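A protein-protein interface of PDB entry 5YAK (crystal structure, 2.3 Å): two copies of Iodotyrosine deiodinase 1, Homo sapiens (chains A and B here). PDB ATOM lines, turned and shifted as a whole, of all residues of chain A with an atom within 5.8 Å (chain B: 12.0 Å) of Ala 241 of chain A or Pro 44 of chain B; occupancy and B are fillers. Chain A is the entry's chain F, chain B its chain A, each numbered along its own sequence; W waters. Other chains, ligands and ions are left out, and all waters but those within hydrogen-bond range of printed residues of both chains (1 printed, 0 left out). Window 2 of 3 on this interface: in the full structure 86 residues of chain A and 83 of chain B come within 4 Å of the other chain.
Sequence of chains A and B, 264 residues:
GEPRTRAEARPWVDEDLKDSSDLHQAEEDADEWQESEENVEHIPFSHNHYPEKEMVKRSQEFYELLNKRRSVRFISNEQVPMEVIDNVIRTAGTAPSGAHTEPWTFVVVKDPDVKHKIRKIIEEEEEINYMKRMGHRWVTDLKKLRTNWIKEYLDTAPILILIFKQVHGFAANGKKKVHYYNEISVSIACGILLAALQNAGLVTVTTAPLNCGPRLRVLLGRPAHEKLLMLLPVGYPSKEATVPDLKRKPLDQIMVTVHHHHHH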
ATOM      1  N   VAL A  72      26.870 -22.163 -11.949  1.00  0.00           N
ATOM      2  CA  VAL A  72      27.027 -21.124 -10.912  1.00  0.00           C
ATOM      3  C   VAL A  72      27.758 -19.941 -11.512  1.00  0.00           C
ATOM      4  O   VAL A  72      28.854 -20.096 -12.067  1.00  0.00           O
ATOM      5  CB  VAL A  72      27.857 -21.682  -9.748  1.00  0.00           C
ATOM      6  CG1 VAL A  72      28.067 -20.635  -8.662  1.00  0.00           C
ATOM      7  CG2 VAL A  72      27.169 -22.913  -9.183  1.00  0.00           C
ATOM      8  N   PHE A  74      28.375 -17.013  -9.856  1.00  0.00           N
ATOM      9  CA  PHE A  74      28.924 -16.201  -8.712  1.00  0.00           C
ATOM     10  C   PHE A  74      29.951 -17.045  -7.947  1.00  0.00           C
ATOM     11  O   PHE A  74      29.594 -17.953  -7.196  1.00  0.00           O
ATOM     12  CB  PHE A  74      27.803 -15.733  -7.775  1.00  0.00           C
ATOM     13  CG  PHE A  74      26.612 -15.187  -8.505  1.00  0.00           C
ATOM     14  CD1 PHE A  74      26.626 -13.883  -8.975  1.00  0.00           C
ATOM     15  CD2 PHE A  74      25.535 -16.019  -8.839  1.00  0.00           C
ATOM     16  CE1 PHE A  74      25.555 -13.378  -9.695  1.00  0.00           C
ATOM     17  CE2 PHE A  74      24.462 -15.522  -9.551  1.00  0.00           C
ATOM     18  CZ  PHE A  74      24.474 -14.199  -9.996  1.00  0.00           C
ATOM     19  N   PRO A 237      31.637 -21.589  -4.975  1.00  0.00           N
ATOM     20  CA  PRO A 237      30.586 -20.605  -5.089  1.00  0.00           C
ATOM     21  C   PRO A 237      30.802 -19.460  -4.102  1.00  0.00           C
ATOM     22  O   PRO A 237      31.497 -19.639  -3.113  1.00  0.00           O
ATOM     23  CB  PRO A 237      29.311 -21.402  -4.755  1.00  0.00           C
ATOM     24  CG  PRO A 237      29.758 -22.602  -4.025  1.00  0.00           C
ATOM     25  CD  PRO A 237      31.163 -22.878  -4.453  1.00  0.00           C
ATOM     26  N   SER A 238      30.249 -18.288  -4.388  1.00  0.00           N
ATOM     27  CA  SER A 238      30.223 -17.215  -3.406  1.00  0.00           C
ATOM     28  C   SER A 238      29.218 -17.562  -2.326  1.00  0.00           C
ATOM     29  O   SER A 238      28.133 -18.121  -2.612  1.00  0.00           O
ATOM     30  CB  SER A 238      29.804 -15.893  -4.052  1.00  0.00           C
ATOM     31  OG  SER A 238      30.717 -15.557  -5.070  1.00  0.00           O
ATOM     32  N   LYS A 239      29.550 -17.169  -1.100  1.00  0.00           N
ATOM     33  CA  LYS A 239      28.607 -17.202   0.008  1.00  0.00           C
ATOM     34  C   LYS A 239      27.198 -16.827  -0.470  1.00  0.00           C
ATOM     35  O   LYS A 239      26.237 -17.533  -0.201  1.00  0.00           O
ATOM     36  CB  LYS A 239      29.056 -16.213   1.089  1.00  0.00           C
ATOM     37  CG  LYS A 239      28.803 -16.696   2.506  1.00  0.00           C
ATOM     38  CD  LYS A 239      29.771 -17.803   2.918  1.00  0.00           C
ATOM     39  CE  LYS A 239      29.996 -17.814   4.428  1.00  0.00           C
ATOM     40  NZ  LYS A 239      28.733 -17.628   5.210  1.00  0.00           N
ATOM     41  N   GLU A 240      27.088 -15.743  -1.229  1.00  0.00           N
ATOM     42  CA  GLU A 240      25.782 -15.235  -1.659  1.00  0.00           C
ATOM     43  C   GLU A 240      25.232 -15.818  -2.996  1.00  0.00           C
ATOM     44  O   GLU A 240      24.268 -15.283  -3.543  1.00  0.00           O
ATOM     45  CB  GLU A 240      25.837 -13.685  -1.724  1.00  0.00           C
ATOM     46  CG  GLU A 240      25.870 -12.990  -0.349  1.00  0.00           C
ATOM     47  CD  GLU A 240      24.787 -13.492   0.641  1.00  0.00           C
ATOM     48  OE1 GLU A 240      23.552 -13.369   0.357  1.00  0.00           O
ATOM     49  OE2 GLU A 240      25.170 -14.006   1.727  1.00  0.00           O
ATOM     50  N   ALA A 241      25.811 -16.913  -3.500  1.00  0.00           N
ATOM     51  CA  ALA A 241      25.517 -17.352  -4.882  1.00  0.00           C
ATOM     52  C   ALA A 241      24.060 -17.778  -5.001  1.00  0.00           C
ATOM     53  O   ALA A 241      23.537 -18.475  -4.144  1.00  0.00           O
ATOM     54  CB  ALA A 241      26.443 -18.488  -5.320  1.00  0.00           C
ATOM     55  N   THR A 242      23.383 -17.310  -6.039  1.00  0.00           N
ATOM     56  CA  THR A 242      22.075 -17.867  -6.362  1.00  0.00           C
ATOM     57  C   THR A 242      22.186 -18.757  -7.628  1.00  0.00           C
ATOM     58  O   THR A 242      23.201 -18.746  -8.348  1.00  0.00           O
ATOM     59  CB  THR A 242      21.048 -16.747  -6.532  1.00  0.00           C
ATOM     60  OG1 THR A 242      21.572 -15.786  -7.435  1.00  0.00           O
ATOM     61  CG2 THR A 242      20.784 -16.039  -5.169  1.00  0.00           C
ATOM     62  N   VAL A 243      21.176 -19.590  -7.823  1.00  0.00           N
ATOM     63  CA  VAL A 243      20.862 -20.145  -9.137  1.00  0.00           C
ATOM     64  C   VAL A 243      19.390 -19.935  -9.406  1.00  0.00           C
ATOM     65  O   VAL A 243      18.600 -19.800  -8.460  1.00  0.00           O
ATOM     66  CB  VAL A 243      21.154 -21.644  -9.227  1.00  0.00           C
ATOM     67  CG1 VAL A 243      22.656 -21.904  -9.087  1.00  0.00           C
ATOM     68  CG2 VAL A 243      20.355 -22.415  -8.184  1.00  0.00           C
ATOM     69  N   GLU B  41      12.205 -17.356 -11.006  1.00  0.00           N
ATOM     70  CA  GLU B  41      12.571 -17.082  -9.566  1.00  0.00           C
ATOM     71  C   GLU B  41      13.943 -17.653  -9.111  1.00  0.00           C
ATOM     72  O   GLU B  41      14.231 -18.819  -9.354  1.00  0.00           O
ATOM     73  CB  GLU B  41      11.477 -17.641  -8.657  1.00  0.00           C
ATOM     74  CG  GLU B  41      11.705 -17.409  -7.175  1.00  0.00           C
ATOM     75  CD  GLU B  41      11.771 -15.938  -6.821  1.00  0.00           C
ATOM     76  OE1 GLU B  41      11.285 -15.098  -7.608  1.00  0.00           O
ATOM     77  OE2 GLU B  41      12.300 -15.619  -5.742  1.00  0.00           O
ATOM     78  N   HIS B  42      14.755 -16.859  -8.404  1.00  0.00           N
ATOM     79  CA  HIS B  42      16.144 -17.256  -8.084  1.00  0.00           C
ATOM     80  C   HIS B  42      16.409 -17.620  -6.624  1.00  0.00           C
ATOM     81  O   HIS B  42      16.053 -16.873  -5.731  1.00  0.00           O
ATOM     82  CB  HIS B  42      17.109 -16.164  -8.530  1.00  0.00           C
ATOM     83  CG  HIS B  42      17.337 -16.150 -10.011  1.00  0.00           C
ATOM     84  ND1 HIS B  42      18.571 -16.401 -10.580  1.00  0.00           N
ATOM     85  CD2 HIS B  42      16.470 -15.997 -11.042  1.00  0.00           C
ATOM     86  CE1 HIS B  42      18.461 -16.359 -11.893  1.00  0.00           C
ATOM     87  NE2 HIS B  42      17.195 -16.125 -12.200  1.00  0.00           N
ATOM     88  N   ILE B  43      17.082 -18.751  -6.399  1.00  0.00           N
ATOM     89  CA  ILE B  43      17.245 -19.306  -5.062  1.00  0.00           C
ATOM     90  C   ILE B  43      18.684 -19.491  -4.630  1.00  0.00           C
ATOM     91  O   ILE B  43      19.566 -19.543  -5.454  1.00  0.00           O
ATOM     92  CB  ILE B  43      16.505 -20.655  -4.877  1.00  0.00           C
ATOM     93  CG1 ILE B  43      17.078 -21.732  -5.793  1.00  0.00           C
ATOM     94  CG2 ILE B  43      14.994 -20.443  -5.054  1.00  0.00           C
ATOM     95  CD1 ILE B  43      16.711 -23.160  -5.401  1.00  0.00           C
ATOM     96  N   PRO B  44      18.917 -19.599  -3.309  1.00  0.00           N
ATOM     97  CA  PRO B  44      20.290 -19.787  -2.834  1.00  0.00           C
ATOM     98  C   PRO B  44      20.897 -21.098  -3.269  1.00  0.00           C
ATOM     99  O   PRO B  44      20.227 -22.127  -3.305  1.00  0.00           O
ATOM    100  CB  PRO B  44      20.154 -19.739  -1.298  1.00  0.00           C
ATOM    101  CG  PRO B  44      18.909 -18.927  -1.064  1.00  0.00           C
ATOM    102  CD  PRO B  44      17.985 -19.279  -2.201  1.00  0.00           C
ATOM    103  N   PHE B  45      22.179 -21.069  -3.588  1.00  0.00           N
ATOM    104  CA  PHE B  45      22.789 -22.242  -4.114  1.00  0.00           C
ATOM    105  C   PHE B  45      23.445 -22.930  -2.963  1.00  0.00           C
ATOM    106  O   PHE B  45      24.325 -22.351  -2.337  1.00  0.00           O
ATOM    107  CB  PHE B  45      23.826 -21.929  -5.187  1.00  0.00           C
ATOM    108  CG  PHE B  45      24.592 -23.138  -5.614  1.00  0.00           C
ATOM    109  CD1 PHE B  45      23.937 -24.202  -6.233  1.00  0.00           C
ATOM    110  CD2 PHE B  45      25.922 -23.273  -5.305  1.00  0.00           C
ATOM    111  CE1 PHE B  45      24.623 -25.350  -6.584  1.00  0.00           C
ATOM    112  CE2 PHE B  45      26.610 -24.429  -5.655  1.00  0.00           C
ATOM    113  CZ  PHE B  45      25.954 -25.465  -6.289  1.00  0.00           C
ATOM    114  N   SER B  46      23.022 -24.168  -2.711  1.00  0.00           N
ATOM    115  CA  SER B  46      23.570 -24.973  -1.629  1.00  0.00           C
ATOM    116  C   SER B  46      24.613 -25.965  -2.171  1.00  0.00           C
ATOM    117  O   SER B  46      24.297 -26.934  -2.873  1.00  0.00           O
ATOM    118  CB  SER B  46      22.443 -25.700  -0.884  1.00  0.00           C
ATOM    119  OG  SER B  46      21.738 -26.566  -1.757  1.00  0.00           O
ATOM    120  N   HIS B  47      25.867 -25.716  -1.824  1.00  0.00           N
ATOM    121  CA  HIS B  47      26.977 -26.498  -2.345  1.00  0.00           C
ATOM    122  C   HIS B  47      27.322 -27.640  -1.420  1.00  0.00           C
ATOM    123  O   HIS B  47      27.133 -27.527  -0.225  1.00  0.00           O
ATOM    124  CB  HIS B  47      28.191 -25.588  -2.471  1.00  0.00           C
ATOM    125  CG  HIS B  47      29.389 -26.256  -3.063  1.00  0.00           C
ATOM    126  ND1 HIS B  47      29.292 -27.270  -3.992  1.00  0.00           N
ATOM    127  CD2 HIS B  47      30.712 -26.027  -2.884  1.00  0.00           C
ATOM    128  CE1 HIS B  47      30.505 -27.640  -4.356  1.00  0.00           C
ATOM    129  NE2 HIS B  47      31.385 -26.901  -3.700  1.00  0.00           N
ATOM    130  N   ASN B  48      27.855 -28.727  -1.963  1.00  0.00           N
ATOM    131  CA  ASN B  48      28.532 -29.737  -1.135  1.00  0.00           C
ATOM    132  C   ASN B  48      30.057 -29.745  -1.308  1.00  0.00           C
ATOM    133  O   ASN B  48      30.592 -30.176  -2.342  1.00  0.00           O
ATOM    134  CB  ASN B  48      27.925 -31.124  -1.357  1.00  0.00           C
ATOM    135  CG  ASN B  48      26.659 -31.335  -0.536  1.00  0.00           C
ATOM    136  OD1 ASN B  48      26.684 -31.209   0.693  1.00  0.00           O
ATOM    137  ND2 ASN B  48      25.545 -31.639  -1.207  1.00  0.00           N
HETATM  138  O   HOH W   1      20.953 -16.972 -10.107  1.00  0.00           O
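Ala 241 of chain A touches two residues of chain B.
Printed residues of chain A within 4 Å of Pro 44 of chain B: Ala 241 (3.7 Å).
Of chain B, only Phe 45 comes within 4 Å of Val 72 of chain A.
No residue of chain B comes within 4 Å of Phe 74 of chain A.
Ser 238 of chain A touches none of the printed residues of chain B.
No residue of chain B comes within 4 Å of Glu 240 of chain A.
Of chain B, only His 42, Ile 43 and Phe 45 come within 4 Å of Val 243 of chain A.
Printed residues of chain A within 4 Å of Phe 45 of chain B: Val 72 (3.9 Å), Pro 237 (3.9 Å), Ala 241 (3.0 Å) and Val 243 (3.9 Å).
Printed residues of chain A within 4 Å of His 42 of chain B: Val 243.
Printed residues of chain A within 4 Å of Ile 43 of chain B: Thr 242 and Val 243.
Printed residues of chain A within 4 Å of His 47 of chain B: Pro 237.
Lys 239 of chain A touches none of the printed residues of chain B.
The nearest printed residue of chain A that does not touch His 42 of chain B is Thr 242 of chain A (4.4 Å).
O of Val 243 of chain A sits at hydrogen-bond distance from N of Ile 43 of chain B.
The backbone NH (N) of Phe 45 of chain B is in hydrogen-bond range of the backbone carbonyl oxygen (O) of Ala 241 of chain A (3.0 Å).
Water W1 lies within hydrogen-bond range of a ring nitrogen (ND1) of His 42 of chain B (2.5 Å), the side-chain hydroxyl (OG1) of Thr 242 of chain A (3.0 Å) and the backbone NH (N) of Val 243 of chain A (3.5 Å).
Hydrophobic or aromatic side chains of chain A that line the printed part of chain B: Val 72, Pro 237 and Val 243.
Along chain A the printed residues that touch a printed residue of chain B span positions 72 to 243.
Of the 8 printed residues of chain B, 5 touch a printed residue of chain A.
Printed residues of chain B that touch a printed residue of chain A: His 42, Ile 43, Pro 44, Phe 45 and His 47.
Hydrophobic or aromatic side chains of chain B that line the printed part of chain A: His 42, Ile 43, Phe 45 and His 47.
Along chain B the printed residues that touch a printed residue of chain A span positions 42 to 47.
Among the printed residues, 9 pairs touch across the chains.
Among the printed residues, no Asp or Glu carboxylate lies within 4 Å of a Lys or Arg side-chain nitrogen of the other chain.
No position is printed for both chains.
Of the 9 pairs that touch across the chains among the printed residues, none has its exchanged pair printed and touching as well.
Among the printed residues, merely in contact across the chains: Thr 242 of chain A with Ile 43 of chain B, Pro 237 of chain A with His 47 of chain B, Val 243 of chain A with His 42 of chain B, Ala 241 of chain A with Pro 44 of chain B, Val 72 of chain A with Phe 45 of chain B, Val 243 of chain A with Phe 45 of chain B and Pro 237 of chain A with Phe 45 of chain B.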
